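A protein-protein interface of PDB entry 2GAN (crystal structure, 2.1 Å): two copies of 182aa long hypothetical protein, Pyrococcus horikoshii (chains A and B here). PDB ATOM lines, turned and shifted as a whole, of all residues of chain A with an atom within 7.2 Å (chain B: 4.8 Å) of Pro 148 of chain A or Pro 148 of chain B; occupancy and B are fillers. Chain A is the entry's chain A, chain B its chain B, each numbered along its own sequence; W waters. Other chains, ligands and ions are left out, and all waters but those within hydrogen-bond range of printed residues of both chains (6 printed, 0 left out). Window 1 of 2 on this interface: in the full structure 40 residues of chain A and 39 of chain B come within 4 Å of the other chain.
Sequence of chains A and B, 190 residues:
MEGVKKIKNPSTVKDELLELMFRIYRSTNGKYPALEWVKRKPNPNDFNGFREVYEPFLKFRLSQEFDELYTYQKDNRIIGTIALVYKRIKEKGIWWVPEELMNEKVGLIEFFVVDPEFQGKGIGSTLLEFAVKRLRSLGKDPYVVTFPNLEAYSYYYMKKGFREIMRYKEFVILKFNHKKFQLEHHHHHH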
ATOM      1  N   THR A 146      21.420  14.319  17.878  1.00  0.00           N
ATOM      2  CA  THR A 146      22.295  15.268  18.544  1.00  0.00           C
ATOM      3  C   THR A 146      22.283  14.962  20.027  1.00  0.00           C
ATOM      4  O   THR A 146      21.323  14.409  20.549  1.00  0.00           O
ATOM      5  CB  THR A 146      21.834  16.721  18.330  1.00  0.00           C
ATOM      6  OG1 THR A 146      20.593  16.918  19.010  1.00  0.00           O
ATOM      7  CG2 THR A 146      21.653  17.005  16.858  1.00  0.00           C
ATOM      8  N   PHE A 147      23.348  15.357  20.697  1.00  0.00           N
ATOM      9  CA  PHE A 147      23.500  15.101  22.114  1.00  0.00           C
ATOM     10  C   PHE A 147      23.550  16.400  22.906  1.00  0.00           C
ATOM     11  O   PHE A 147      24.589  17.044  22.994  1.00  0.00           O
ATOM     12  CB  PHE A 147      24.774  14.301  22.295  1.00  0.00           C
ATOM     13  CG  PHE A 147      24.890  13.156  21.330  1.00  0.00           C
ATOM     14  CD1 PHE A 147      24.047  12.054  21.442  1.00  0.00           C
ATOM     15  CD2 PHE A 147      25.823  13.188  20.299  1.00  0.00           C
ATOM     16  CE1 PHE A 147      24.130  10.999  20.545  1.00  0.00           C
ATOM     17  CE2 PHE A 147      25.916  12.138  19.393  1.00  0.00           C
ATOM     18  CZ  PHE A 147      25.069  11.037  19.516  1.00  0.00           C
ATOM     19  N   PRO A 148      22.423  16.787  23.519  1.00  0.00           N
ATOM     20  CA  PRO A 148      22.369  18.030  24.296  1.00  0.00           C
ATOM     21  C   PRO A 148      23.371  18.173  25.443  1.00  0.00           C
ATOM     22  O   PRO A 148      23.768  19.288  25.774  1.00  0.00           O
ATOM     23  CB  PRO A 148      20.906  18.088  24.761  1.00  0.00           C
ATOM     24  CG  PRO A 148      20.514  16.654  24.841  1.00  0.00           C
ATOM     25  CD  PRO A 148      21.153  16.045  23.617  1.00  0.00           C
ATOM     26  N   ASN A 149      23.805  17.066  26.038  1.00  0.00           N
ATOM     27  CA  ASN A 149      24.754  17.171  27.140  1.00  0.00           C
ATOM     28  C   ASN A 149      26.103  17.711  26.653  1.00  0.00           C
ATOM     29  O   ASN A 149      27.021  17.911  27.444  1.00  0.00           O
ATOM     30  CB  ASN A 149      24.958  15.812  27.827  1.00  0.00           C
ATOM     31  CG  ASN A 149      25.982  14.946  27.118  1.00  0.00           C
ATOM     32  OD1 ASN A 149      25.691  14.320  26.101  1.00  0.00           O
ATOM     33  ND2 ASN A 149      27.198  14.920  27.650  1.00  0.00           N
ATOM     34  N   LEU A 150      26.219  17.945  25.348  1.00  0.00           N
ATOM     35  CA  LEU A 150      27.453  18.465  24.790  1.00  0.00           C
ATOM     36  C   LEU A 150      27.411  19.982  24.629  1.00  0.00           C
ATOM     37  O   LEU A 150      28.363  20.592  24.132  1.00  0.00           O
ATOM     38  CB  LEU A 150      27.753  17.786  23.454  1.00  0.00           C
ATOM     39  CG  LEU A 150      27.946  16.270  23.627  1.00  0.00           C
ATOM     40  CD1 LEU A 150      28.284  15.642  22.281  1.00  0.00           C
ATOM     41  CD2 LEU A 150      29.080  16.000  24.632  1.00  0.00           C
ATOM     42  N   GLU A 151      26.303  20.587  25.043  1.00  0.00           N
ATOM     43  CA  GLU A 151      26.167  22.041  24.966  1.00  0.00           C
ATOM     44  C   GLU A 151      27.361  22.608  25.718  1.00  0.00           C
ATOM     45  O   GLU A 151      27.702  22.130  26.799  1.00  0.00           O
ATOM     46  CB  GLU A 151      24.858  22.487  25.620  1.00  0.00           C
ATOM     47  CG  GLU A 151      24.572  23.988  25.545  1.00  0.00           C
ATOM     48  CD  GLU A 151      25.245  24.780  26.659  1.00  0.00           C
ATOM     49  OE1 GLU A 151      25.356  24.265  27.795  1.00  0.00           O
ATOM     50  OE2 GLU A 151      25.650  25.933  26.408  1.00  0.00           O
ATOM     51  N   ALA A 152      27.993  23.623  25.140  1.00  0.00           N
ATOM     52  CA  ALA A 152      29.189  24.242  25.709  1.00  0.00           C
ATOM     53  C   ALA A 152      29.220  24.508  27.215  1.00  0.00           C
ATOM     54  O   ALA A 152      30.137  24.055  27.904  1.00  0.00           O
ATOM     55  CB  ALA A 152      29.501  25.526  24.959  1.00  0.00           C
ATOM     56  N   SER A 154      27.072  23.499  29.699  1.00  0.00           N
ATOM     57  CA  SER A 154      26.831  22.316  30.493  1.00  0.00           C
ATOM     58  C   SER A 154      28.086  21.449  30.538  1.00  0.00           C
ATOM     59  O   SER A 154      28.506  21.018  31.604  1.00  0.00           O
ATOM     60  CB  SER A 154      25.661  21.520  29.922  1.00  0.00           C
ATOM     61  OG  SER A 154      25.315  20.483  30.813  1.00  0.00           O
ATOM     62  N   TYR A 155      28.686  21.216  29.380  1.00  0.00           N
ATOM     63  CA  TYR A 155      29.894  20.409  29.287  1.00  0.00           C
ATOM     64  C   TYR A 155      30.990  20.972  30.194  1.00  0.00           C
ATOM     65  O   TYR A 155      31.624  20.240  30.955  1.00  0.00           O
ATOM     66  CB  TYR A 155      30.393  20.386  27.841  1.00  0.00           C
ATOM     67  CG  TYR A 155      31.499  19.388  27.577  1.00  0.00           C
ATOM     68  CD1 TYR A 155      31.231  18.022  27.511  1.00  0.00           C
ATOM     69  CD2 TYR A 155      32.812  19.817  27.362  1.00  0.00           C
ATOM     70  CE1 TYR A 155      32.247  17.100  27.227  1.00  0.00           C
ATOM     71  CE2 TYR A 155      33.829  18.906  27.081  1.00  0.00           C
ATOM     72  CZ  TYR A 155      33.530  17.547  27.013  1.00  0.00           C
ATOM     73  OH  TYR A 155      34.522  16.652  26.714  1.00  0.00           O
ATOM     74  N   ARG A 167      15.747  19.768  34.571  1.00  0.00           N
ATOM     75  CA  ARG A 167      15.757  20.245  33.198  1.00  0.00           C
ATOM     76  C   ARG A 167      14.392  20.748  32.749  1.00  0.00           C
ATOM     77  O   ARG A 167      13.989  20.527  31.606  1.00  0.00           O
ATOM     78  CB  ARG A 167      16.247  19.145  32.245  1.00  0.00           C
ATOM     79  CG  ARG A 167      15.499  17.820  32.322  1.00  0.00           C
ATOM     80  CD  ARG A 167      16.025  16.943  33.459  1.00  0.00           C
ATOM     81  NE  ARG A 167      15.497  15.578  33.402  1.00  0.00           N
ATOM     82  CZ  ARG A 167      14.220  15.254  33.595  1.00  0.00           C
ATOM     83  NH1 ARG A 167      13.843  13.985  33.518  1.00  0.00           N
ATOM     84  NH2 ARG A 167      13.324  16.193  33.876  1.00  0.00           N
ATOM     85  N   LYS A 169      11.387  23.023  31.370  1.00  0.00           N
ATOM     86  CA  LYS A 169      11.286  23.977  30.270  1.00  0.00           C
ATOM     87  C   LYS A 169      12.467  23.795  29.323  1.00  0.00           C
ATOM     88  O   LYS A 169      13.074  22.724  29.274  1.00  0.00           O
ATOM     89  CB  LYS A 169      11.267  25.414  30.804  1.00  0.00           C
ATOM     90  CG  LYS A 169       9.879  26.024  31.010  1.00  0.00           C
ATOM     91  CD  LYS A 169       9.044  25.265  32.030  1.00  0.00           C
ATOM     92  CE  LYS A 169       7.799  26.056  32.397  1.00  0.00           C
ATOM     93  NZ  LYS A 169       8.148  27.436  32.842  1.00  0.00           N
ATOM     94  N   GLU A 170      12.793  24.847  28.578  1.00  0.00           N
ATOM     95  CA  GLU A 170      13.902  24.801  27.631  1.00  0.00           C
ATOM     96  C   GLU A 170      15.257  24.921  28.333  1.00  0.00           C
ATOM     97  O   GLU A 170      16.276  25.144  27.674  1.00  0.00           O
ATOM     98  CB  GLU A 170      13.794  25.937  26.608  1.00  0.00           C
ATOM     99  CG  GLU A 170      12.434  26.091  25.935  1.00  0.00           C
ATOM    100  CD  GLU A 170      12.513  26.918  24.653  1.00  0.00           C
ATOM    101  OE1 GLU A 170      13.119  28.019  24.674  1.00  0.00           O
ATOM    102  OE2 GLU A 170      11.958  26.470  23.622  1.00  0.00           O
ATOM    103  N   PHE A 171      15.276  24.763  29.655  1.00  0.00           N
ATOM    104  CA  PHE A 171      16.519  24.895  30.401  1.00  0.00           C
ATOM    105  C   PHE A 171      16.953  23.649  31.152  1.00  0.00           C
ATOM    106  O   PHE A 171      16.160  22.751  31.409  1.00  0.00           O
ATOM    107  CB  PHE A 171      16.422  26.045  31.412  1.00  0.00           C
ATOM    108  CG  PHE A 171      15.474  27.134  31.011  1.00  0.00           C
ATOM    109  CD1 PHE A 171      14.112  27.017  31.263  1.00  0.00           C
ATOM    110  CD2 PHE A 171      15.938  28.273  30.368  1.00  0.00           C
ATOM    111  CE1 PHE A 171      13.229  28.024  30.885  1.00  0.00           C
ATOM    112  CE2 PHE A 171      15.061  29.287  29.984  1.00  0.00           C
ATOM    113  CZ  PHE A 171      13.704  29.160  30.242  1.00  0.00           C
ATOM    114  N   VAL A 172      18.229  23.622  31.519  1.00  0.00           N
ATOM    115  CA  VAL A 172      18.799  22.515  32.271  1.00  0.00           C
ATOM    116  C   VAL A 172      19.549  23.077  33.473  1.00  0.00           C
ATOM    117  O   VAL A 172      20.660  23.578  33.326  1.00  0.00           O
ATOM    118  CB  VAL A 172      19.796  21.711  31.421  1.00  0.00           C
ATOM    119  CG1 VAL A 172      20.445  20.639  32.279  1.00  0.00           C
ATOM    120  CG2 VAL A 172      19.091  21.087  30.228  1.00  0.00           C
ATOM    121  N   ILE A 173      18.948  22.998  34.655  1.00  0.00           N
ATOM    122  CA  ILE A 173      19.594  23.518  35.855  1.00  0.00           C
ATOM    123  C   ILE A 173      20.641  22.561  36.419  1.00  0.00           C
ATOM    124  O   ILE A 173      20.389  21.361  36.554  1.00  0.00           O
ATOM    125  CB  ILE A 173      18.569  23.817  36.968  1.00  0.00           C
ATOM    126  CG1 ILE A 173      17.557  24.862  36.493  1.00  0.00           C
ATOM    127  CG2 ILE A 173      19.283  24.322  38.209  1.00  0.00           C
ATOM    128  CD1 ILE A 173      16.403  24.285  35.718  1.00  0.00           C
ATOM    129  N   THR B 146      21.560  26.336  32.064  1.00  0.00           N
ATOM    130  CA  THR B 146      22.098  26.159  30.721  1.00  0.00           C
ATOM    131  C   THR B 146      20.965  25.956  29.713  1.00  0.00           C
ATOM    132  O   THR B 146      19.835  25.662  30.096  1.00  0.00           O
ATOM    133  CB  THR B 146      23.047  24.945  30.677  1.00  0.00           C
ATOM    134  OG1 THR B 146      22.297  23.742  30.893  1.00  0.00           O
ATOM    135  CG2 THR B 146      24.104  25.061  31.774  1.00  0.00           C
ATOM    136  N   PHE B 147      21.268  26.123  28.432  1.00  0.00           N
ATOM    137  CA  PHE B 147      20.273  25.975  27.374  1.00  0.00           C
ATOM    138  C   PHE B 147      20.708  24.872  26.396  1.00  0.00           C
ATOM    139  O   PHE B 147      21.506  25.112  25.491  1.00  0.00           O
ATOM    140  CB  PHE B 147      20.122  27.313  26.638  1.00  0.00           C
ATOM    141  CG  PHE B 147      19.958  28.493  27.563  1.00  0.00           C
ATOM    142  CD1 PHE B 147      18.799  28.653  28.318  1.00  0.00           C
ATOM    143  CD2 PHE B 147      20.979  29.428  27.709  1.00  0.00           C
ATOM    144  CE1 PHE B 147      18.662  29.724  29.207  1.00  0.00           C
ATOM    145  CE2 PHE B 147      20.850  30.501  28.594  1.00  0.00           C
ATOM    146  CZ  PHE B 147      19.690  30.647  29.343  1.00  0.00           C
ATOM    147  N   PRO B 148      20.182  23.646  26.567  1.00  0.00           N
ATOM    148  CA  PRO B 148      20.526  22.508  25.699  1.00  0.00           C
ATOM    149  C   PRO B 148      20.419  22.722  24.187  1.00  0.00           C
ATOM    150  O   PRO B 148      21.179  22.130  23.426  1.00  0.00           O
ATOM    151  CB  PRO B 148      19.614  21.386  26.209  1.00  0.00           C
ATOM    152  CG  PRO B 148      18.478  22.126  26.894  1.00  0.00           C
ATOM    153  CD  PRO B 148      19.187  23.252  27.578  1.00  0.00           C
ATOM    154  N   ASN B 149      19.489  23.567  23.758  1.00  0.00           N
ATOM    155  CA  ASN B 149      19.306  23.861  22.341  1.00  0.00           C
ATOM    156  C   ASN B 149      20.513  24.553  21.703  1.00  0.00           C
ATOM    157  O   ASN B 149      20.640  24.598  20.474  1.00  0.00           O
ATOM    158  CB  ASN B 149      18.060  24.732  22.141  1.00  0.00           C
ATOM    159  CG  ASN B 149      16.826  23.916  21.800  1.00  0.00           C
ATOM    160  OD1 ASN B 149      16.465  22.974  22.510  1.00  0.00           O
ATOM    161  ND2 ASN B 149      16.170  24.276  20.704  1.00  0.00           N
ATOM    162  N   LEU B 150      21.391  25.104  22.534  1.00  0.00           N
ATOM    163  CA  LEU B 150      22.581  25.784  22.032  1.00  0.00           C
ATOM    164  C   LEU B 150      23.733  24.815  21.743  1.00  0.00           C
ATOM    165  O   LEU B 150      24.840  25.245  21.391  1.00  0.00           O
ATOM    166  CB  LEU B 150      23.030  26.864  23.026  1.00  0.00           C
ATOM    167  CG  LEU B 150      22.538  28.311  22.809  1.00  0.00           C
ATOM    168  CD1 LEU B 150      21.207  28.342  22.095  1.00  0.00           C
ATOM    169  CD2 LEU B 150      22.462  29.031  24.161  1.00  0.00           C
ATOM    170  N   GLU B 151      23.475  23.513  21.880  1.00  0.00           N
ATOM    171  CA  GLU B 151      24.498  22.507  21.587  1.00  0.00           C
ATOM    172  C   GLU B 151      24.880  22.699  20.117  1.00  0.00           C
ATOM    173  O   GLU B 151      24.008  22.804  19.256  1.00  0.00           O
ATOM    174  CB  GLU B 151      23.946  21.095  21.839  1.00  0.00           C
ATOM    175  CG  GLU B 151      24.931  19.965  21.548  1.00  0.00           C
ATOM    176  CD  GLU B 151      24.915  19.550  20.089  1.00  0.00           C
ATOM    177  OE1 GLU B 151      25.999  19.411  19.487  1.00  0.00           O
ATOM    178  OE2 GLU B 151      23.815  19.358  19.542  1.00  0.00           O
ATOM    179  N   GLU B 170      19.501  10.954  26.685  1.00  0.00           N
ATOM    180  CA  GLU B 170      20.863  11.139  26.193  1.00  0.00           C
ATOM    181  C   GLU B 170      20.974  11.705  24.776  1.00  0.00           C
ATOM    182  O   GLU B 170      22.075  11.993  24.316  1.00  0.00           O
ATOM    183  CB  GLU B 170      21.633   9.816  26.276  1.00  0.00           C
ATOM    184  CG  GLU B 170      21.713   9.242  27.693  1.00  0.00           C
ATOM    185  CD  GLU B 170      22.459   7.916  27.755  1.00  0.00           C
ATOM    186  OE1 GLU B 170      22.201   7.039  26.899  1.00  0.00           O
ATOM    187  OE2 GLU B 170      23.290   7.745  28.673  1.00  0.00           O
ATOM    188  N   PHE B 171      19.852  11.875  24.081  1.00  0.00           N
ATOM    189  CA  PHE B 171      19.920  12.416  22.728  1.00  0.00           C
ATOM    190  C   PHE B 171      18.588  12.967  22.252  1.00  0.00           C
ATOM    191  O   PHE B 171      17.552  12.707  22.846  1.00  0.00           O
ATOM    192  CB  PHE B 171      20.399  11.337  21.745  1.00  0.00           C
ATOM    193  CG  PHE B 171      19.507  10.119  21.692  1.00  0.00           C
ATOM    194  CD1 PHE B 171      19.728   9.037  22.542  1.00  0.00           C
ATOM    195  CD2 PHE B 171      18.426  10.071  20.813  1.00  0.00           C
ATOM    196  CE1 PHE B 171      18.883   7.921  22.521  1.00  0.00           C
ATOM    197  CE2 PHE B 171      17.572   8.962  20.782  1.00  0.00           C
ATOM    198  CZ  PHE B 171      17.799   7.882  21.642  1.00  0.00           C
ATOM    199  N   VAL B 172      18.620  13.742  21.173  1.00  0.00           N
ATOM    200  CA  VAL B 172      17.389  14.285  20.617  1.00  0.00           C
ATOM    201  C   VAL B 172      17.423  14.114  19.102  1.00  0.00           C
ATOM    202  O   VAL B 172      18.403  14.462  18.447  1.00  0.00           O
ATOM    203  CB  VAL B 172      17.180  15.779  21.022  1.00  0.00           C
ATOM    204  CG1 VAL B 172      18.502  16.520  21.028  1.00  0.00           C
ATOM    205  CG2 VAL B 172      16.201  16.446  20.060  1.00  0.00           C
HETATM  206  O   HOH W   1      21.758  18.184  21.179  1.00  0.00           O
HETATM  207  O   HOH W   2      25.456  16.437  19.094  1.00  0.00           O
HETATM  208  O   HOH W   3      23.849  27.272  27.779  1.00  0.00           O
HETATM  209  O   HOH W   4      22.433  22.912  28.013  1.00  0.00           O
HETATM  210  O   HOH W   5      27.017  25.077  22.748  1.00  0.00           O
HETATM  211  O   HOH W   6      23.239  14.444  25.494  1.00  0.00           O
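The side-chain carboxylate (OE1) of Glu 151 of chain A lies within hydrogen-bond range of the backbone NH (N) of Ser 154 of chain A.
Thr 146 of chain A touches Val 172 of chain B, and with the chains exchanged Val 172 of chain A touches Thr 146 of chain B.
Leu 150 of chain A touches Glu 151 of chain B, and with the chains exchanged Glu 151 of chain A touches Leu 150 of chain B.
Glu 151 of chain B touches its own counterpart, Glu 151 of chain A.
Glu 170 of chain A touches Pro 148 of chain B, but with the chains exchanged Pro 148 of chain A does not touch Glu 170 of chain B (4.2 Å).
Positions printed for both chains: 146, 147, 148, 149, 150, 151, 170, 171 and 172.
O of Thr 146 of chain A sits at hydrogen-bond distance from N of Val 172 of chain B (2.9 Å).
The backbone carbonyl oxygen (O) of Val 172 of chain A lies within hydrogen-bond range of the side-chain hydroxyl (OG1) of Thr 146 of chain B (2.9 Å).
Hydrophobic or aromatic side chains of chain B that line the printed part of chain A: Phe 147, Pro 148, Phe 171 and Val 172.
Along chain B the printed residues that touch a printed residue of chain A span positions 146 to 172.
Of the 15 printed residues of chain A, 9 touch a printed residue of chain B.
Water W6 bridges the side-chain amide oxygen of Asn 149 of chain A (2.5 Å) and the backbone carbonyl oxygen of Glu 170 of chain B (3.0 Å).
Water W5 lies within hydrogen-bond range of the backbone carbonyl oxygen of Leu 150 of chain B (2.6 Å) and the backbone NH of Ala 152 of chain A (3.0 Å).
Water W3 lies within hydrogen-bond range of the side-chain carboxylate (OE2) of Glu 151 of chain A and the backbone NH (N) of Phe 147 of chain B.
Water W1 lies within hydrogen-bond range of OG1 of Thr 146 of chain A, OE2 of Glu 151 of chain B and N of Phe 147 of chain A.
Water W2 bridges N of Phe 147 of chain A and OE1 of Glu 151 of chain B.
Water W4 lies within hydrogen-bond range of OG1 of Thr 146 of chain B (3.0 Å), OE1 of Glu 151 of chain A (3.2 Å) and N of Phe 147 of chain B (3.4 Å).
Among the printed residues, pairs that only touch across the chains: Thr 146 of chain A with Glu 151 of chain B, Thr 146 of chain A with Phe 171 of chain B, Phe 147 of chain A with Glu 151 of chain B, Phe 147 of chain A with Glu 170 of chain B, Phe 147 of chain A with Phe 171 of chain B, Pro 148 of chain A with Pro 148 of chain B, Pro 148 of chain A with Phe 171 of chain B, Pro 148 of chain A with Val 172 of chain B, Leu 150 of chain A with Glu 151 of chain B, Glu 151 of chain A with Thr 146 of chain B, Glu 151 of chain A with Phe 147 of chain B, Glu 151 of chain A with Leu 150 of chain B, Glu 151 of chain A with Glu 151 of chain B, Ser 154 of chain A with Thr 146 of chain B, Glu 170 of chain A with Pro 148 of chain B, Phe 171 of chain A with Thr 146 of chain B, Phe 171 of chain A with Phe 147 of chain B and Val 172 of chain A with Pro 148 of chain B.
Pro 148 of chain A touches just these residues of chain B: Pro 148, Phe 171 and Val 172.
Pro 148 of chain B touches three residues of chain A.
Of the printed residues of chain B, Phe 147 of chain A touches Glu 151 (3.3 Å), Glu 170 (3.5 Å) and Phe 171 (3.7 Å).
Printed residues of chain B within 4 Å of Thr 146 of chain A: Glu 151 (3.5 Å), Phe 171 (3.3 Å) and Val 172 (2.9 Å).
Of the printed residues of chain A, Val 172 of chain B touches Thr 146 (2.9 Å) and Pro 148 (3.7 Å).
Printed residues of chain B within 4 Å of Glu 151 of chain A: Thr 146, Phe 147, Leu 150 and Glu 151.
Asn 149 of chain A touches none of the printed residues of chain B.
Ala 152 of chain A touches none of the printed residues of chain B.
The nearest printed residue of chain B that does not touch Pro 148 of chain A is Glu 170 of chain B (4.2 Å).
The nearest residue of chain A that does not touch Pro 148 of chain B is Phe 171 of chain A (4.2 Å).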
